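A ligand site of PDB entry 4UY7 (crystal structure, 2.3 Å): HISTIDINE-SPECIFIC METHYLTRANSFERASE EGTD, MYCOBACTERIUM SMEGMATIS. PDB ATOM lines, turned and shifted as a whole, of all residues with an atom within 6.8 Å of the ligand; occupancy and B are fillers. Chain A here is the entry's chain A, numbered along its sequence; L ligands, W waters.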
ATOM      1  N   PHE A  37     -15.099  27.396   6.514  1.00  0.00           N
ATOM      2  CA  PHE A  37     -16.009  27.930   5.484  1.00  0.00           C
ATOM      3  C   PHE A  37     -17.244  27.026   5.315  1.00  0.00           C
ATOM      4  O   PHE A  37     -18.260  27.476   4.789  1.00  0.00           O
ATOM      5  CB  PHE A  37     -15.310  28.061   4.128  1.00  0.00           C
ATOM      6  CG  PHE A  37     -14.390  29.245   4.005  1.00  0.00           C
ATOM      7  CD1 PHE A  37     -14.770  30.496   4.477  1.00  0.00           C
ATOM      8  CD2 PHE A  37     -13.139  29.104   3.401  1.00  0.00           C
ATOM      9  CE1 PHE A  37     -13.919  31.597   4.349  1.00  0.00           C
ATOM     10  CE2 PHE A  37     -12.284  30.196   3.272  1.00  0.00           C
ATOM     11  CZ  PHE A  37     -12.673  31.444   3.741  1.00  0.00           C
ATOM     12  N   TYR A  38     -17.146  25.774   5.750  1.00  0.00           N
ATOM     13  CA  TYR A  38     -18.079  24.758   5.237  1.00  0.00           C
ATOM     14  C   TYR A  38     -19.142  24.284   6.238  1.00  0.00           C
ATOM     15  O   TYR A  38     -19.347  23.075   6.407  1.00  0.00           O
ATOM     16  CB  TYR A  38     -17.265  23.574   4.679  1.00  0.00           C
ATOM     17  CG  TYR A  38     -16.374  24.034   3.542  1.00  0.00           C
ATOM     18  CD1 TYR A  38     -16.868  24.190   2.250  1.00  0.00           C
ATOM     19  CD2 TYR A  38     -15.045  24.383   3.777  1.00  0.00           C
ATOM     20  CE1 TYR A  38     -16.048  24.655   1.212  1.00  0.00           C
ATOM     21  CE2 TYR A  38     -14.224  24.836   2.747  1.00  0.00           C
ATOM     22  CZ  TYR A  38     -14.731  24.974   1.479  1.00  0.00           C
ATOM     23  OH  TYR A  38     -13.907  25.437   0.463  1.00  0.00           O
ATOM     24  N   PHE A  46     -20.482  27.578  -1.687  1.00  0.00           N
ATOM     25  CA  PHE A  46     -19.342  27.061  -2.466  1.00  0.00           C
ATOM     26  C   PHE A  46     -19.871  26.293  -3.671  1.00  0.00           C
ATOM     27  O   PHE A  46     -19.299  26.356  -4.760  1.00  0.00           O
ATOM     28  CB  PHE A  46     -18.442  26.162  -1.624  1.00  0.00           C
ATOM     29  CG  PHE A  46     -17.451  25.393  -2.447  1.00  0.00           C
ATOM     30  CD1 PHE A  46     -16.285  26.007  -2.911  1.00  0.00           C
ATOM     31  CD2 PHE A  46     -17.689  24.071  -2.789  1.00  0.00           C
ATOM     32  CE1 PHE A  46     -15.381  25.307  -3.690  1.00  0.00           C
ATOM     33  CE2 PHE A  46     -16.792  23.356  -3.563  1.00  0.00           C
ATOM     34  CZ  PHE A  46     -15.633  23.976  -4.016  1.00  0.00           C
ATOM     35  N   ILE A  49     -20.414  28.640  -6.105  1.00  0.00           N
ATOM     36  CA  ILE A  49     -19.161  29.085  -6.697  1.00  0.00           C
ATOM     37  C   ILE A  49     -18.757  28.176  -7.874  1.00  0.00           C
ATOM     38  O   ILE A  49     -18.293  28.669  -8.921  1.00  0.00           O
ATOM     39  CB  ILE A  49     -18.020  29.155  -5.652  1.00  0.00           C
ATOM     40  CG1 ILE A  49     -18.146  30.467  -4.852  1.00  0.00           C
ATOM     41  CG2 ILE A  49     -16.633  29.077  -6.321  1.00  0.00           C
ATOM     42  CD1 ILE A  49     -17.361  30.484  -3.547  1.00  0.00           C
ATOM     43  N   TYR A  55     -15.283  31.009 -12.293  1.00  0.00           N
ATOM     44  CA  TYR A  55     -14.662  29.945 -11.501  1.00  0.00           C
ATOM     45  C   TYR A  55     -14.542  28.666 -12.317  1.00  0.00           C
ATOM     46  O   TYR A  55     -15.357  27.751 -12.170  1.00  0.00           O
ATOM     47  CB  TYR A  55     -15.428  29.692 -10.179  1.00  0.00           C
ATOM     48  CG  TYR A  55     -14.666  28.740  -9.270  1.00  0.00           C
ATOM     49  CD1 TYR A  55     -13.586  29.195  -8.519  1.00  0.00           C
ATOM     50  CD2 TYR A  55     -14.977  27.391  -9.225  1.00  0.00           C
ATOM     51  CE1 TYR A  55     -12.852  28.330  -7.717  1.00  0.00           C
ATOM     52  CE2 TYR A  55     -14.257  26.499  -8.421  1.00  0.00           C
ATOM     53  CZ  TYR A  55     -13.194  26.980  -7.680  1.00  0.00           C
ATOM     54  OH  TYR A  55     -12.480  26.097  -6.897  1.00  0.00           O
ATOM     55  N   PRO A  57     -12.268  26.105 -12.214  1.00  0.00           N
ATOM     56  CA  PRO A  57     -11.654  24.828 -11.809  1.00  0.00           C
ATOM     57  C   PRO A  57     -12.576  23.618 -11.650  1.00  0.00           C
ATOM     58  O   PRO A  57     -12.182  22.532 -12.083  1.00  0.00           O
ATOM     59  CB  PRO A  57     -11.003  25.165 -10.462  1.00  0.00           C
ATOM     60  CG  PRO A  57     -10.699  26.615 -10.562  1.00  0.00           C
ATOM     61  CD  PRO A  57     -11.885  27.175 -11.260  1.00  0.00           C
ATOM     62  N   GLY A 160     -11.415  18.136  -6.424  1.00  0.00           N
ATOM     63  CA  GLY A 160     -11.845  19.424  -5.883  1.00  0.00           C
ATOM     64  C   GLY A 160     -10.709  20.399  -5.641  1.00  0.00           C
ATOM     65  O   GLY A 160     -10.929  21.477  -5.056  1.00  0.00           O
ATOM     66  N   SER A 161      -9.503  20.050  -6.090  1.00  0.00           N
ATOM     67  CA  SER A 161      -8.268  20.827  -5.852  1.00  0.00           C
ATOM     68  C   SER A 161      -8.117  21.396  -4.425  1.00  0.00           C
ATOM     69  O   SER A 161      -7.528  22.466  -4.230  1.00  0.00           O
ATOM     70  CB  SER A 161      -8.170  21.970  -6.872  1.00  0.00           C
ATOM     71  OG  SER A 161      -9.431  22.562  -7.117  1.00  0.00           O
ATOM     72  N   THR A 162      -8.626  20.642  -3.447  1.00  0.00           N
ATOM     73  CA  THR A 162      -8.517  20.954  -2.013  1.00  0.00           C
ATOM     74  C   THR A 162      -7.090  21.027  -1.545  1.00  0.00           C
ATOM     75  O   THR A 162      -6.744  21.855  -0.707  1.00  0.00           O
ATOM     76  CB  THR A 162      -9.199  19.882  -1.163  1.00  0.00           C
ATOM     77  OG1 THR A 162     -10.313  19.333  -1.879  1.00  0.00           O
ATOM     78  CG2 THR A 162      -9.614  20.456   0.172  1.00  0.00           C
ATOM     79  N   ILE A 163      -6.261  20.132  -2.101  1.00  0.00           N
ATOM     80  CA  ILE A 163      -4.853  20.013  -1.754  1.00  0.00           C
ATOM     81  C   ILE A 163      -4.116  21.341  -1.897  1.00  0.00           C
ATOM     82  O   ILE A 163      -3.090  21.547  -1.269  1.00  0.00           O
ATOM     83  CB  ILE A 163      -4.187  18.952  -2.625  1.00  0.00           C
ATOM     84  CG1 ILE A 163      -2.834  18.537  -2.039  1.00  0.00           C
ATOM     85  CG2 ILE A 163      -4.079  19.418  -4.095  1.00  0.00           C
ATOM     86  CD1 ILE A 163      -2.687  17.045  -1.929  1.00  0.00           C
ATOM     87  N   GLY A 164      -4.643  22.221  -2.756  1.00  0.00           N
ATOM     88  CA  GLY A 164      -4.098  23.543  -2.985  1.00  0.00           C
ATOM     89  C   GLY A 164      -4.407  24.506  -1.845  1.00  0.00           C
ATOM     90  O   GLY A 164      -3.724  25.521  -1.700  1.00  0.00           O
ATOM     91  N   ASN A 165      -5.416  24.194  -1.038  1.00  0.00           N
ATOM     92  CA  ASN A 165      -5.728  25.056   0.121  1.00  0.00           C
ATOM     93  C   ASN A 165      -4.776  24.827   1.314  1.00  0.00           C
ATOM     94  O   ASN A 165      -4.881  25.517   2.325  1.00  0.00           O
ATOM     95  CB  ASN A 165      -7.186  24.845   0.570  1.00  0.00           C
ATOM     96  CG  ASN A 165      -8.206  25.188  -0.522  1.00  0.00           C
ATOM     97  OD1 ASN A 165      -9.063  24.391  -0.849  1.00  0.00           O
ATOM     98  ND2 ASN A 165      -8.095  26.399  -1.088  1.00  0.00           N
ATOM     99  N   ASP A 193      -4.883  22.473  -9.853  1.00  0.00           N
ATOM    100  CA  ASP A 193      -5.074  23.633 -10.716  1.00  0.00           C
ATOM    101  C   ASP A 193      -3.715  24.207 -11.082  1.00  0.00           C
ATOM    102  O   ASP A 193      -2.836  24.253 -10.222  1.00  0.00           O
ATOM    103  CB  ASP A 193      -5.930  24.676 -10.019  1.00  0.00           C
ATOM    104  CG  ASP A 193      -6.455  25.718 -10.959  1.00  0.00           C
ATOM    105  OD1 ASP A 193      -6.471  25.466 -12.185  1.00  0.00           O
ATOM    106  OD2 ASP A 193      -6.874  26.789 -10.473  1.00  0.00           O
ATOM    107  N   ALA A 204     -11.250  34.503 -10.695  1.00  0.00           N
ATOM    108  CA  ALA A 204     -11.872  33.248 -10.261  1.00  0.00           C
ATOM    109  C   ALA A 204     -12.172  33.265  -8.760  1.00  0.00           C
ATOM    110  O   ALA A 204     -13.069  32.546  -8.308  1.00  0.00           O
ATOM    111  CB  ALA A 204     -10.980  32.063 -10.596  1.00  0.00           C
ATOM    112  N   TYR A 205     -11.420  34.064  -8.017  1.00  0.00           N
ATOM    113  CA  TYR A 205     -11.541  34.127  -6.562  1.00  0.00           C
ATOM    114  C   TYR A 205     -12.117  35.458  -6.064  1.00  0.00           C
ATOM    115  O   TYR A 205     -12.062  35.782  -4.865  1.00  0.00           O
ATOM    116  CB  TYR A 205     -10.181  33.829  -5.928  1.00  0.00           C
ATOM    117  CG  TYR A 205      -9.790  32.373  -6.156  1.00  0.00           C
ATOM    118  CD1 TYR A 205     -10.224  31.377  -5.262  1.00  0.00           C
ATOM    119  CD2 TYR A 205      -9.079  31.988  -7.291  1.00  0.00           C
ATOM    120  CE1 TYR A 205      -9.898  30.044  -5.470  1.00  0.00           C
ATOM    121  CE2 TYR A 205      -8.761  30.644  -7.525  1.00  0.00           C
ATOM    122  CZ  TYR A 205      -9.169  29.677  -6.608  1.00  0.00           C
ATOM    123  OH  TYR A 205      -8.851  28.354  -6.837  1.00  0.00           O
ATOM    124  N   THR A 212     -18.269  34.760  -4.096  1.00  0.00           N
ATOM    125  CA  THR A 212     -17.055  34.432  -3.339  1.00  0.00           C
ATOM    126  C   THR A 212     -16.934  35.311  -2.087  1.00  0.00           C
ATOM    127  O   THR A 212     -16.658  34.814  -0.993  1.00  0.00           O
ATOM    128  CB  THR A 212     -15.788  34.597  -4.212  1.00  0.00           C
ATOM    129  OG1 THR A 212     -15.874  33.733  -5.356  1.00  0.00           O
ATOM    130  CG2 THR A 212     -14.533  34.260  -3.403  1.00  0.00           C
ATOM    131  N   PHE A 215     -19.186  34.082   0.465  1.00  0.00           N
ATOM    132  CA  PHE A 215     -18.538  32.848   0.920  1.00  0.00           C
ATOM    133  C   PHE A 215     -17.438  33.175   1.935  1.00  0.00           C
ATOM    134  O   PHE A 215     -17.332  32.536   2.993  1.00  0.00           O
ATOM    135  CB  PHE A 215     -17.964  32.100  -0.301  1.00  0.00           C
ATOM    136  CG  PHE A 215     -17.261  30.823   0.043  1.00  0.00           C
ATOM    137  CD1 PHE A 215     -17.971  29.682   0.383  1.00  0.00           C
ATOM    138  CD2 PHE A 215     -15.879  30.746  -0.022  1.00  0.00           C
ATOM    139  CE1 PHE A 215     -17.335  28.480   0.682  1.00  0.00           C
ATOM    140  CE2 PHE A 215     -15.223  29.552   0.275  1.00  0.00           C
ATOM    141  CZ  PHE A 215     -15.963  28.419   0.629  1.00  0.00           C
ATOM    142  N   MET A 251      -7.036  34.723  -0.168  1.00  0.00           N
ATOM    143  CA  MET A 251      -8.246  35.458   0.204  1.00  0.00           C
ATOM    144  C   MET A 251      -8.076  36.140   1.556  1.00  0.00           C
ATOM    145  O   MET A 251      -7.665  35.515   2.533  1.00  0.00           O
ATOM    146  CB  MET A 251      -9.475  34.535   0.255  1.00  0.00           C
ATOM    147  CG  MET A 251      -9.759  33.882  -1.090  1.00  0.00           C
ATOM    148  SD  MET A 251     -11.480  33.456  -1.408  1.00  0.00           S
ATOM    149  CE  MET A 251     -11.883  32.552   0.086  1.00  0.00           C
ATOM    150  N   GLU A 281      -7.680  32.149   3.539  1.00  0.00           N
ATOM    151  CA  GLU A 281      -7.428  31.032   2.626  1.00  0.00           C
ATOM    152  C   GLU A 281      -6.281  31.308   1.659  1.00  0.00           C
ATOM    153  O   GLU A 281      -6.072  32.438   1.219  1.00  0.00           O
ATOM    154  CB  GLU A 281      -8.677  30.698   1.812  1.00  0.00           C
ATOM    155  CG  GLU A 281      -8.607  29.382   1.048  1.00  0.00           C
ATOM    156  CD  GLU A 281      -9.893  29.093   0.287  1.00  0.00           C
ATOM    157  OE1 GLU A 281     -10.206  29.853  -0.665  1.00  0.00           O
ATOM    158  OE2 GLU A 281     -10.594  28.116   0.653  1.00  0.00           O
ATOM    159  N   VAL A 282      -5.528  30.271   1.337  1.00  0.00           N
ATOM    160  CA  VAL A 282      -4.617  30.348   0.198  1.00  0.00           C
ATOM    161  C   VAL A 282      -5.080  29.292  -0.796  1.00  0.00           C
ATOM    162  O   VAL A 282      -5.666  28.284  -0.404  1.00  0.00           O
ATOM    163  CB  VAL A 282      -3.153  30.117   0.600  1.00  0.00           C
ATOM    164  CG1 VAL A 282      -2.700  31.214   1.579  1.00  0.00           C
ATOM    165  CG2 VAL A 282      -2.989  28.733   1.206  1.00  0.00           C
ATOM    166  N   SER A 283      -4.880  29.549  -2.085  1.00  0.00           N
ATOM    167  CA  SER A 283      -5.201  28.553  -3.100  1.00  0.00           C
ATOM    168  C   SER A 283      -3.961  28.427  -4.001  1.00  0.00           C
ATOM    169  O   SER A 283      -3.698  29.273  -4.858  1.00  0.00           O
ATOM    170  CB  SER A 283      -6.449  28.966  -3.880  1.00  0.00           C
ATOM    171  OG  SER A 283      -6.950  27.907  -4.673  1.00  0.00           O
ATOM    172  N   CYS A 284      -3.193  27.362  -3.773  1.00  0.00           N
ATOM    173  CA  CYS A 284      -1.913  27.177  -4.473  1.00  0.00           C
ATOM    174  C   CYS A 284      -2.081  26.599  -5.875  1.00  0.00           C
ATOM    175  O   CYS A 284      -2.747  25.585  -6.069  1.00  0.00           O
ATOM    176  CB  CYS A 284      -0.988  26.270  -3.658  1.00  0.00           C
ATOM    177  SG  CYS A 284      -0.566  26.952  -2.035  1.00  0.00           S
ATOM    178  N   LYS A 285      -1.445  27.253  -6.850  1.00  0.00           N
ATOM    179  CA  LYS A 285      -1.515  26.810  -8.228  1.00  0.00           C
ATOM    180  C   LYS A 285      -0.208  26.130  -8.646  1.00  0.00           C
ATOM    181  O   LYS A 285       0.873  26.582  -8.299  1.00  0.00           O
ATOM    182  CB  LYS A 285      -1.846  28.013  -9.121  1.00  0.00           C
ATOM    183  CG  LYS A 285      -3.091  28.799  -8.641  1.00  0.00           C
ATOM    184  CD  LYS A 285      -4.351  27.982  -8.799  1.00  0.00           C
ATOM    185  CE  LYS A 285      -5.466  28.460  -7.862  1.00  0.00           C
ATOM    186  NZ  LYS A 285      -6.572  27.439  -7.734  1.00  0.00           N
HETATM  187  N1  LIG L   1     -10.918  24.415  -3.356  1.00  0.00           N
HETATM  188  C1  LIG L   1     -11.440  25.709  -3.784  1.00  0.00           C
HETATM  189  C2  LIG L   1     -10.325  26.516  -4.433  1.00  0.00           C
HETATM  190  O1  LIG L   1     -10.451  26.857  -5.625  1.00  0.00           O
HETATM  191  C3  LIG L   1     -12.043  26.494  -2.616  1.00  0.00           C
HETATM  192  C4  LIG L   1     -12.457  27.901  -2.958  1.00  0.00           C
HETATM  193  N2  LIG L   1     -12.017  28.999  -2.258  1.00  0.00           N
HETATM  194  C5  LIG L   1     -13.273  28.370  -3.933  1.00  0.00           C
HETATM  195  C6  LIG L   1     -12.536  30.089  -2.793  1.00  0.00           C
HETATM  196  N3  LIG L   1     -13.302  29.735  -3.805  1.00  0.00           N
HETATM  197  O2  LIG L   1      -9.303  26.806  -3.787  1.00  0.00           O
HETATM  198  O   HOH W   1     -13.955  31.486  -5.624  1.00  0.00           O
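O1 of the ligand sits at hydrogen-bond distance from OH of Tyr 205, 2.5 Å away. O1 of the ligand lies within hydrogen-bond range of OH of Tyr 55. N2 of the ligand sits at hydrogen-bond distance from OE1 of Glu 281 (2.6 Å). An oxygen (O2) of the ligand sits at hydrogen-bond distance from the side-chain hydroxyl (OG) of Ser 283, at 2.7 Å. An oxygen (O2) of the ligand is in hydrogen-bond range of the side-chain amide nitrogen (ND2) of Asn 165 (3.0 Å). The backbone carbonyl oxygen (O) of Gly 160 lies within hydrogen-bond range of a nitrogen (N1) of the ligand (3.4 Å).
OG of Ser 283 lies within hydrogen-bond range of OH of Tyr 205 (2.9 Å). NZ of Lys 285 is in hydrogen-bond range of OH of Tyr 205, at 2.6 Å. The side-chain amide nitrogen (ND2) of Asn 165 is in hydrogen-bond range of the side-chain carboxylate (OE2) of Glu 281. N of Met 251 is in hydrogen-bond range of O of Glu 281 (2.8 Å). The side-chain hydroxyl (OG) of Ser 283 lies within hydrogen-bond range of the side-chain amino group (NZ) of Lys 285, 3.1 Å away. The side-chain amide oxygen of Asn 165 lies close to the backbone carbonyl oxygen of Thr 162, at 3.4 Å. The side-chain amide nitrogen of Asn 165 lies within hydrogen-bond range of the backbone carbonyl oxygen of Val 282 (3.1 Å).
Residues that only touch the ligand: Phe 46 (3.7 Å), Tyr 38 (3.8 Å) and Met 251 (3.8 Å). Of the 23 residues printed, 9 come within 4 Å of the ligand. The nearest printed residue that does not touch the ligand is Ser 161 (4.01 Å).
Water W1 lies within hydrogen-bond range of a nitrogen (N3) of the ligand (2.6 Å), the side-chain hydroxyl (OG1) of Thr 212 (3.0 Å) and the backbone carbonyl oxygen (O) of Ala 204 (3.0 Å).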
